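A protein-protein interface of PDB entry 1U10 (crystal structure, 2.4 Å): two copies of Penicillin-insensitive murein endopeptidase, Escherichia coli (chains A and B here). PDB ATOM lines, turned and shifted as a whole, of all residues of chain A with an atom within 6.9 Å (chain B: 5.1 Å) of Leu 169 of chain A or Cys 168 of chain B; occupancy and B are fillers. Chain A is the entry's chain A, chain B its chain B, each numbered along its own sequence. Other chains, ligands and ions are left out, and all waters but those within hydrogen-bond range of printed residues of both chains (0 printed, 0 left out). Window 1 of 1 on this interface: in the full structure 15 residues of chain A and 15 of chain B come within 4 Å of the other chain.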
ATOM      1  N   PHE A 142      36.464  -1.144  -7.679  1.00  0.00           N
ATOM      2  CA  PHE A 142      35.074  -1.185  -7.264  1.00  0.00           C
ATOM      3  C   PHE A 142      34.240  -1.612  -8.479  1.00  0.00           C
ATOM      4  O   PHE A 142      33.422  -2.532  -8.383  1.00  0.00           O
ATOM      5  CB  PHE A 142      34.624   0.207  -6.798  1.00  0.00           C
ATOM      6  CG  PHE A 142      33.129   0.346  -6.674  1.00  0.00           C
ATOM      7  CD1 PHE A 142      32.480  -0.097  -5.528  1.00  0.00           C
ATOM      8  CD2 PHE A 142      32.359   0.864  -7.730  1.00  0.00           C
ATOM      9  CE1 PHE A 142      31.091  -0.037  -5.410  1.00  0.00           C
ATOM     10  CE2 PHE A 142      30.955   0.928  -7.622  1.00  0.00           C
ATOM     11  CZ  PHE A 142      30.325   0.471  -6.448  1.00  0.00           C
ATOM     12  N   LYS A 164      34.812  -5.929   1.239  1.00  0.00           N
ATOM     13  CA  LYS A 164      33.361  -5.807   1.156  1.00  0.00           C
ATOM     14  C   LYS A 164      32.927  -4.554   1.928  1.00  0.00           C
ATOM     15  O   LYS A 164      31.991  -3.856   1.543  1.00  0.00           O
ATOM     16  CB  LYS A 164      32.650  -7.014   1.749  1.00  0.00           C
ATOM     17  CG  LYS A 164      31.175  -6.859   1.542  1.00  0.00           C
ATOM     18  CD  LYS A 164      30.370  -8.024   1.982  1.00  0.00           C
ATOM     19  CE  LYS A 164      28.936  -7.820   1.529  1.00  0.00           C
ATOM     20  NZ  LYS A 164      28.133  -9.005   1.890  1.00  0.00           N
ATOM     21  N   GLN A 165      33.615  -4.282   3.025  1.00  0.00           N
ATOM     22  CA  GLN A 165      33.290  -3.113   3.820  1.00  0.00           C
ATOM     23  C   GLN A 165      33.404  -1.871   2.927  1.00  0.00           C
ATOM     24  O   GLN A 165      32.496  -1.035   2.891  1.00  0.00           O
ATOM     25  CB  GLN A 165      34.235  -3.017   5.022  1.00  0.00           C
ATOM     26  CG  GLN A 165      34.040  -1.777   5.871  1.00  0.00           C
ATOM     27  CD  GLN A 165      35.195  -0.799   5.735  1.00  0.00           C
ATOM     28  OE1 GLN A 165      35.182   0.286   6.332  1.00  0.00           O
ATOM     29  NE2 GLN A 165      36.206  -1.179   4.945  1.00  0.00           N
ATOM     30  N   GLN A 166      34.515  -1.771   2.201  1.00  0.00           N
ATOM     31  CA  GLN A 166      34.740  -0.642   1.305  1.00  0.00           C
ATOM     32  C   GLN A 166      33.641  -0.576   0.236  1.00  0.00           C
ATOM     33  O   GLN A 166      33.105   0.504  -0.051  1.00  0.00           O
ATOM     34  CB  GLN A 166      36.115  -0.763   0.654  1.00  0.00           C
ATOM     35  CG  GLN A 166      36.481   0.394  -0.249  1.00  0.00           C
ATOM     36  CD  GLN A 166      36.342   1.743   0.453  1.00  0.00           C
ATOM     37  OE1 GLN A 166      36.863   1.943   1.559  1.00  0.00           O
ATOM     38  NE2 GLN A 166      35.635   2.673  -0.187  1.00  0.00           N
ATOM     39  N   LEU A 167      33.282  -1.729  -0.330  1.00  0.00           N
ATOM     40  CA  LEU A 167      32.249  -1.762  -1.352  1.00  0.00           C
ATOM     41  C   LEU A 167      30.932  -1.269  -0.780  1.00  0.00           C
ATOM     42  O   LEU A 167      30.168  -0.604  -1.478  1.00  0.00           O
ATOM     43  CB  LEU A 167      32.052  -3.179  -1.915  1.00  0.00           C
ATOM     44  CG  LEU A 167      33.242  -3.890  -2.564  1.00  0.00           C
ATOM     45  CD1 LEU A 167      32.788  -5.189  -3.128  1.00  0.00           C
ATOM     46  CD2 LEU A 167      33.850  -3.046  -3.645  1.00  0.00           C
ATOM     47  N   CYS A 168      30.660  -1.595   0.487  1.00  0.00           N
ATOM     48  CA  CYS A 168      29.415  -1.160   1.120  1.00  0.00           C
ATOM     49  C   CYS A 168      29.322   0.369   1.240  1.00  0.00           C
ATOM     50  O   CYS A 168      28.230   0.941   1.156  1.00  0.00           O
ATOM     51  CB  CYS A 168      29.253  -1.796   2.505  1.00  0.00           C
ATOM     52  SG  CYS A 168      28.894  -3.586   2.549  1.00  0.00           S
ATOM     53  N   LEU A 169      30.467   1.018   1.430  1.00  0.00           N
ATOM     54  CA  LEU A 169      30.521   2.470   1.542  1.00  0.00           C
ATOM     55  C   LEU A 169      30.364   3.151   0.176  1.00  0.00           C
ATOM     56  O   LEU A 169      29.646   4.148   0.053  1.00  0.00           O
ATOM     57  CB  LEU A 169      31.846   2.888   2.184  1.00  0.00           C
ATOM     58  CG  LEU A 169      32.036   2.388   3.618  1.00  0.00           C
ATOM     59  CD1 LEU A 169      33.497   2.570   4.096  1.00  0.00           C
ATOM     60  CD2 LEU A 169      31.060   3.134   4.507  1.00  0.00           C
ATOM     61  N   ASP A 170      31.013   2.598  -0.846  1.00  0.00           N
ATOM     62  CA  ASP A 170      30.961   3.167  -2.185  1.00  0.00           C
ATOM     63  C   ASP A 170      29.697   2.866  -2.963  1.00  0.00           C
ATOM     64  O   ASP A 170      29.401   3.568  -3.918  1.00  0.00           O
ATOM     65  CB  ASP A 170      32.128   2.671  -3.051  1.00  0.00           C
ATOM     66  CG  ASP A 170      33.493   3.019  -2.478  1.00  0.00           C
ATOM     67  OD1 ASP A 170      33.552   3.925  -1.607  1.00  0.00           O
ATOM     68  OD2 ASP A 170      34.503   2.391  -2.914  1.00  0.00           O
ATOM     69  N   ALA A 171      28.959   1.839  -2.572  1.00  0.00           N
ATOM     70  CA  ALA A 171      27.784   1.454  -3.345  1.00  0.00           C
ATOM     71  C   ALA A 171      26.720   2.518  -3.558  1.00  0.00           C
ATOM     72  O   ALA A 171      26.243   2.681  -4.676  1.00  0.00           O
ATOM     73  CB  ALA A 171      27.145   0.163  -2.769  1.00  0.00           C
ATOM     74  N   GLY A 172      26.357   3.255  -2.519  1.00  0.00           N
ATOM     75  CA  GLY A 172      25.319   4.261  -2.672  1.00  0.00           C
ATOM     76  C   GLY A 172      23.953   3.594  -2.719  1.00  0.00           C
ATOM     77  O   GLY A 172      23.700   2.643  -1.984  1.00  0.00           O
ATOM     78  N   ARG A 175      22.811  -0.982  -4.721  1.00  0.00           N
ATOM     79  CA  ARG A 175      23.572  -1.929  -3.891  1.00  0.00           C
ATOM     80  C   ARG A 175      23.091  -3.369  -3.771  1.00  0.00           C
ATOM     81  O   ARG A 175      23.723  -4.181  -3.088  1.00  0.00           O
ATOM     82  CB  ARG A 175      23.734  -1.330  -2.477  1.00  0.00           C
ATOM     83  CG  ARG A 175      22.436  -0.802  -1.863  1.00  0.00           C
ATOM     84  CD  ARG A 175      22.668   0.234  -0.742  1.00  0.00           C
ATOM     85  NE  ARG A 175      23.540  -0.245   0.341  1.00  0.00           N
ATOM     86  CZ  ARG A 175      24.747   0.256   0.618  1.00  0.00           C
ATOM     87  NH1 ARG A 175      25.231   1.268  -0.097  1.00  0.00           N
ATOM     88  NH2 ARG A 175      25.489  -0.277   1.591  1.00  0.00           N
ATOM     89  N   LEU A 178      25.413  -6.274  -3.815  1.00  0.00           N
ATOM     90  CA  LEU A 178      26.273  -6.530  -2.677  1.00  0.00           C
ATOM     91  C   LEU A 178      25.965  -7.864  -2.018  1.00  0.00           C
ATOM     92  O   LEU A 178      26.825  -8.471  -1.378  1.00  0.00           O
ATOM     93  CB  LEU A 178      26.160  -5.391  -1.672  1.00  0.00           C
ATOM     94  CG  LEU A 178      26.817  -4.080  -2.121  1.00  0.00           C
ATOM     95  CD1 LEU A 178      26.652  -3.037  -1.029  1.00  0.00           C
ATOM     96  CD2 LEU A 178      28.311  -4.309  -2.395  1.00  0.00           C
ATOM     97  N   ASP A 214      22.029  -6.539   1.978  1.00  0.00           N
ATOM     98  CA  ASP A 214      23.386  -6.319   1.496  1.00  0.00           C
ATOM     99  C   ASP A 214      24.446  -7.011   2.357  1.00  0.00           C
ATOM    100  O   ASP A 214      25.586  -7.160   1.940  1.00  0.00           O
ATOM    101  CB  ASP A 214      23.697  -4.816   1.353  1.00  0.00           C
ATOM    102  CG  ASP A 214      23.515  -4.030   2.643  1.00  0.00           C
ATOM    103  OD1 ASP A 214      23.833  -4.545   3.737  1.00  0.00           O
ATOM    104  OD2 ASP A 214      23.074  -2.865   2.553  1.00  0.00           O
ATOM    105  N   CYS A 216      25.911  -5.940   4.887  1.00  0.00           N
ATOM    106  CA  CYS A 216      26.887  -4.991   5.399  1.00  0.00           C
ATOM    107  C   CYS A 216      26.720  -4.794   6.906  1.00  0.00           C
ATOM    108  O   CYS A 216      27.507  -4.103   7.541  1.00  0.00           O
ATOM    109  CB  CYS A 216      26.723  -3.645   4.680  1.00  0.00           C
ATOM    110  SG  CYS A 216      26.891  -3.699   2.857  1.00  0.00           S
ATOM    111  N   LYS B 164      30.237   8.029  11.266  1.00  0.00           N
ATOM    112  CA  LYS B 164      29.379   8.038  10.083  1.00  0.00           C
ATOM    113  C   LYS B 164      29.588   6.776   9.265  1.00  0.00           C
ATOM    114  O   LYS B 164      28.658   6.274   8.619  1.00  0.00           O
ATOM    115  CB  LYS B 164      29.632   9.244   9.181  1.00  0.00           C
ATOM    116  CG  LYS B 164      28.779   9.154   7.928  1.00  0.00           C
ATOM    117  CD  LYS B 164      28.715  10.436   7.149  1.00  0.00           C
ATOM    118  CE  LYS B 164      27.741  10.245   6.010  1.00  0.00           C
ATOM    119  NZ  LYS B 164      27.577  11.466   5.199  1.00  0.00           N
ATOM    120  N   GLN B 165      30.818   6.279   9.281  1.00  0.00           N
ATOM    121  CA  GLN B 165      31.160   5.060   8.570  1.00  0.00           C
ATOM    122  C   GLN B 165      30.361   3.878   9.155  1.00  0.00           C
ATOM    123  O   GLN B 165      29.837   3.035   8.409  1.00  0.00           O
ATOM    124  CB  GLN B 165      32.678   4.833   8.663  1.00  0.00           C
ATOM    125  CG  GLN B 165      33.212   3.555   8.029  1.00  0.00           C
ATOM    126  CD  GLN B 165      33.550   2.463   9.064  1.00  0.00           C
ATOM    127  OE1 GLN B 165      33.926   1.343   8.690  1.00  0.00           O
ATOM    128  NE2 GLN B 165      33.424   2.788  10.365  1.00  0.00           N
ATOM    129  N   GLN B 166      30.236   3.820  10.476  1.00  0.00           N
ATOM    130  CA  GLN B 166      29.481   2.729  11.085  1.00  0.00           C
ATOM    131  C   GLN B 166      28.008   2.890  10.741  1.00  0.00           C
ATOM    132  O   GLN B 166      27.289   1.908  10.627  1.00  0.00           O
ATOM    133  CB  GLN B 166      29.667   2.715  12.601  1.00  0.00           C
ATOM    134  CG  GLN B 166      28.902   1.638  13.331  1.00  0.00           C
ATOM    135  CD  GLN B 166      29.284   0.251  12.883  1.00  0.00           C
ATOM    136  OE1 GLN B 166      30.411   0.016  12.460  1.00  0.00           O
ATOM    137  NE2 GLN B 166      28.351  -0.688  12.984  1.00  0.00           N
ATOM    138  N   LEU B 167      27.565   4.128  10.568  1.00  0.00           N
ATOM    139  CA  LEU B 167      26.166   4.406  10.212  1.00  0.00           C
ATOM    140  C   LEU B 167      25.884   3.991   8.760  1.00  0.00           C
ATOM    141  O   LEU B 167      24.831   3.429   8.442  1.00  0.00           O
ATOM    142  CB  LEU B 167      25.844   5.909  10.371  1.00  0.00           C
ATOM    143  CG  LEU B 167      25.817   6.545  11.767  1.00  0.00           C
ATOM    144  CD1 LEU B 167      25.502   8.029  11.667  1.00  0.00           C
ATOM    145  CD2 LEU B 167      24.773   5.851  12.615  1.00  0.00           C
ATOM    146  N   CYS B 168      26.830   4.294   7.877  1.00  0.00           N
ATOM    147  CA  CYS B 168      26.689   3.961   6.472  1.00  0.00           C
ATOM    148  C   CYS B 168      26.529   2.454   6.356  1.00  0.00           C
ATOM    149  O   CYS B 168      25.713   1.971   5.578  1.00  0.00           O
ATOM    150  CB  CYS B 168      27.921   4.407   5.682  1.00  0.00           C
ATOM    151  SG  CYS B 168      28.136   6.199   5.413  1.00  0.00           S
ATOM    152  N   LEU B 169      27.294   1.721   7.160  1.00  0.00           N
ATOM    153  CA  LEU B 169      27.225   0.265   7.128  1.00  0.00           C
ATOM    154  C   LEU B 169      25.907  -0.303   7.605  1.00  0.00           C
ATOM    155  O   LEU B 169      25.406  -1.240   6.993  1.00  0.00           O
ATOM    156  CB  LEU B 169      28.364  -0.354   7.940  1.00  0.00           C
ATOM    157  CG  LEU B 169      29.770  -0.223   7.329  1.00  0.00           C
ATOM    158  CD1 LEU B 169      30.812  -0.768   8.289  1.00  0.00           C
ATOM    159  CD2 LEU B 169      29.848  -0.942   6.008  1.00  0.00           C
ATOM    160  N   ASP B 170      25.333   0.258   8.667  1.00  0.00           N
ATOM    161  CA  ASP B 170      24.074  -0.254   9.217  1.00  0.00           C
ATOM    162  C   ASP B 170      22.779   0.278   8.588  1.00  0.00           C
ATOM    163  O   ASP B 170      21.711  -0.272   8.835  1.00  0.00           O
ATOM    164  CB  ASP B 170      23.994   0.012  10.735  1.00  0.00           C
ATOM    165  CG  ASP B 170      25.201  -0.537  11.520  1.00  0.00           C
ATOM    166  OD1 ASP B 170      26.002  -1.319  10.958  1.00  0.00           O
ATOM    167  OD2 ASP B 170      25.335  -0.183  12.720  1.00  0.00           O
ATOM    168  N   ALA B 171      22.868   1.331   7.785  1.00  0.00           N
ATOM    169  CA  ALA B 171      21.680   1.945   7.189  1.00  0.00           C
ATOM    170  C   ALA B 171      20.845   1.076   6.271  1.00  0.00           C
ATOM    171  O   ALA B 171      19.625   1.222   6.236  1.00  0.00           O
ATOM    172  CB  ALA B 171      22.060   3.219   6.469  1.00  0.00           C
ATOM    173  N   GLY B 172      21.479   0.185   5.521  1.00  0.00           N
ATOM    174  CA  GLY B 172      20.706  -0.665   4.631  1.00  0.00           C
ATOM    175  C   GLY B 172      19.990   0.133   3.557  1.00  0.00           C
ATOM    176  O   GLY B 172      20.623   0.937   2.875  1.00  0.00           O
ATOM    177  N   ARG B 175      18.336   5.142   3.766  1.00  0.00           N
ATOM    178  CA  ARG B 175      19.561   5.903   3.994  1.00  0.00           C
ATOM    179  C   ARG B 175      19.663   7.331   3.452  1.00  0.00           C
ATOM    180  O   ARG B 175      20.745   7.912   3.459  1.00  0.00           O
ATOM    181  CB  ARG B 175      20.760   5.092   3.505  1.00  0.00           C
ATOM    182  CG  ARG B 175      20.784   4.900   2.024  1.00  0.00           C
ATOM    183  CD  ARG B 175      21.620   3.692   1.629  1.00  0.00           C
ATOM    184  NE  ARG B 175      23.053   3.852   1.882  1.00  0.00           N
ATOM    185  CZ  ARG B 175      23.782   2.997   2.599  1.00  0.00           C
ATOM    186  NH1 ARG B 175      23.212   1.930   3.133  1.00  0.00           N
ATOM    187  NH2 ARG B 175      25.084   3.199   2.776  1.00  0.00           N
ATOM    188  N   LEU B 178      21.216   9.913   5.761  1.00  0.00           N
ATOM    189  CA  LEU B 178      22.672   9.986   5.902  1.00  0.00           C
ATOM    190  C   LEU B 178      23.265  11.290   5.380  1.00  0.00           C
ATOM    191  O   LEU B 178      24.309  11.734   5.848  1.00  0.00           O
ATOM    192  CB  LEU B 178      23.333   8.812   5.190  1.00  0.00           C
ATOM    193  CG  LEU B 178      23.095   7.458   5.857  1.00  0.00           C
ATOM    194  CD1 LEU B 178      23.678   6.341   4.982  1.00  0.00           C
ATOM    195  CD2 LEU B 178      23.736   7.462   7.261  1.00  0.00           C
ATOM    196  N   ASP B 214      24.294   9.839   0.042  1.00  0.00           N
ATOM    197  CA  ASP B 214      24.601   9.458   1.411  1.00  0.00           C
ATOM    198  C   ASP B 214      25.968   9.952   1.866  1.00  0.00           C
ATOM    199  O   ASP B 214      26.244   9.985   3.056  1.00  0.00           O
ATOM    200  CB  ASP B 214      24.515   7.933   1.584  1.00  0.00           C
ATOM    201  CG  ASP B 214      25.559   7.169   0.759  1.00  0.00           C
ATOM    202  OD1 ASP B 214      26.634   7.731   0.437  1.00  0.00           O
ATOM    203  OD2 ASP B 214      25.302   5.984   0.453  1.00  0.00           O
ATOM    204  N   CYS B 216      28.675   8.517   1.704  1.00  0.00           N
ATOM    205  CA  CYS B 216      29.457   7.421   2.251  1.00  0.00           C
ATOM    206  C   CYS B 216      30.700   6.979   1.491  1.00  0.00           C
ATOM    207  O   CYS B 216      31.495   6.200   2.022  1.00  0.00           O
ATOM    208  CB  CYS B 216      28.547   6.217   2.436  1.00  0.00           C
ATOM    209  SG  CYS B 216      27.213   6.525   3.632  1.00  0.00           S
ATOM    210  N   GLY B 217      30.869   7.468   0.261  1.00  0.00           N
ATOM    211  CA  GLY B 217      32.003   7.067  -0.549  1.00  0.00           C
ATOM    212  C   GLY B 217      33.236   7.937  -0.461  1.00  0.00           C
ATOM    213  O   GLY B 217      33.824   8.092   0.601  1.00  0.00           O
ATOM    214  N   LEU B 220      33.681  10.862   2.317  1.00  0.00           N
ATOM    215  CA  LEU B 220      33.917  10.303   3.639  1.00  0.00           C
ATOM    216  C   LEU B 220      35.323   9.745   3.695  1.00  0.00           C
ATOM    217  O   LEU B 220      36.036   9.908   4.687  1.00  0.00           O
ATOM    218  CB  LEU B 220      32.915   9.189   3.942  1.00  0.00           C
ATOM    219  CG  LEU B 220      33.069   8.505   5.306  1.00  0.00           C
ATOM    220  CD1 LEU B 220      32.641   9.467   6.409  1.00  0.00           C
ATOM    221  CD2 LEU B 220      32.215   7.235   5.353  1.00  0.00           C
ATOM    222  N   GLN B 221      35.717   9.096   2.609  1.00  0.00           N
ATOM    223  CA  GLN B 221      37.026   8.489   2.497  1.00  0.00           C
ATOM    224  C   GLN B 221      38.166   9.486   2.599  1.00  0.00           C
ATOM    225  O   GLN B 221      39.231   9.165   3.112  1.00  0.00           O
ATOM    226  CB  GLN B 221      37.131   7.747   1.177  1.00  0.00           C
ATOM    227  CG  GLN B 221      37.754   6.375   1.307  1.00  0.00           C
ATOM    228  CD  GLN B 221      36.995   5.339   0.501  1.00  0.00           C
ATOM    229  OE1 GLN B 221      35.756   5.236   0.607  1.00  0.00           O
ATOM    230  NE2 GLN B 221      37.724   4.561  -0.311  1.00  0.00           N
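Of chain B, only Cys 168 (3.6 Å), Cys 216 (3.3 Å) and Gly 217 (3.5 Å) come within 4 Å of Leu 169 of chain A.
Of chain A, only Leu 169 (3.6 Å) comes within 4 Å of Cys 168 of chain B.
Of the printed residues of chain B, Asp 170 of chain A touches Gly 217 and Gln 221.
Of the printed residues of chain B, Gln 165 of chain A touches Gln 165 (2.9 Å).
Leu 178 of chain B touches none of the printed residues of chain A.
Of the 16 printed residues of chain B, 9 touch a printed residue of chain A.
Of the 14 printed residues of chain A, 9 touch a printed residue of chain B.
Hydrophobic or aromatic side chains of chain A within 4 Å of the printed part of chain B: Leu 169.
Along chain A the printed residues that touch a printed residue of chain B span positions 165 to 216.
Among the printed residues, 12 pairs touch across the chains.
Among the printed residues, no Asp or Glu carboxylate lies within 4 Å of a Lys or Arg side-chain nitrogen of the other chain.
Gln 165 of chain B touches its own counterpart, Gln 165 of chain A.
Leu 169 of chain A touches Cys 216 of chain B, and with the chains exchanged Cys 216 of chain A touches Leu 169 of chain B.
Gly 172 of chain A touches Asp 214 of chain B, and with the chains exchanged Asp 214 of chain A touches Gly 172 of chain B.
Arg 175 of chain B touches its own counterpart, Arg 175 of chain A.
Positions printed for both chains: 164, 165, 166, 167, 168, 169, 170, 171, 172, 175, 178, 214 and 216.
The side-chain amide oxygen (OE1) of Gln 165 of chain B lies close to the side-chain amide oxygen (OE1) of Gln 165 of chain A (2.9 Å).
NE2 of Gln 166 of chain A sits at hydrogen-bond distance from OE1 of Gln 221 of chain B, 2.7 Å away.
The side-chain carboxylate (OD1) of Asp 170 of chain A sits close to the side-chain amide oxygen (OE1) of Gln 221 of chain B, at 3.4 Å.
O of Leu 169 of chain A lies close to O of Cys 216 of chain B (3.4 Å).
The guanidinium group (NH2) of Arg 175 of chain B sits close to the guanidinium group (NH1) of Arg 175 of chain A.
Cys 168 of chain A touches Leu 169 of chain B.
Cys 168 of chain B touches Leu 169 of chain A (CB to CD2, 3.6 Å).
Gly 217 of chain B touches Leu 169 of chain A.
OD1 of Asp 170 of chain A touches CA of Gly 217 of chain B (3.7 Å).
Gly 172 of chain A touches Asp 214 of chain B (CA to OD2, 3.6 Å).
CA of Gly 172 of chain B touches OD2 of Asp 214 of chain A, 3.8 Å away.
O of Leu 169 of chain B touches CB of Cys 216 of chain A (3.6 Å).
NZ of Lys 164 of chain A is in hydrogen-bond range of O of Asp 214 of chain A.
The side-chain carboxylate (OD2) of Asp 214 of chain A is in salt-bridge range of the guanidinium group (NE) of Arg 175 of chain A (3.5 Å).
The backbone carbonyl oxygen (O) of Asp 214 of chain B lies within hydrogen-bond range of the side-chain amino group (NZ) of Lys 164 of chain B, at 2.9 Å.
The backbone carbonyl oxygen (O) of Cys 168 of chain B sits at hydrogen-bond distance from the guanidinium group (NH2) of Arg 175 of chain B (3.1 Å).
SG of Cys 216 of chain B forms a disulfide with SG of Cys 168 of chain B, at 2.0 Å.
The backbone carbonyl oxygen (O) of Gly 217 of chain B lies close to the side-chain amide oxygen (OE1) of Gln 221 of chain B (3.4 Å).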
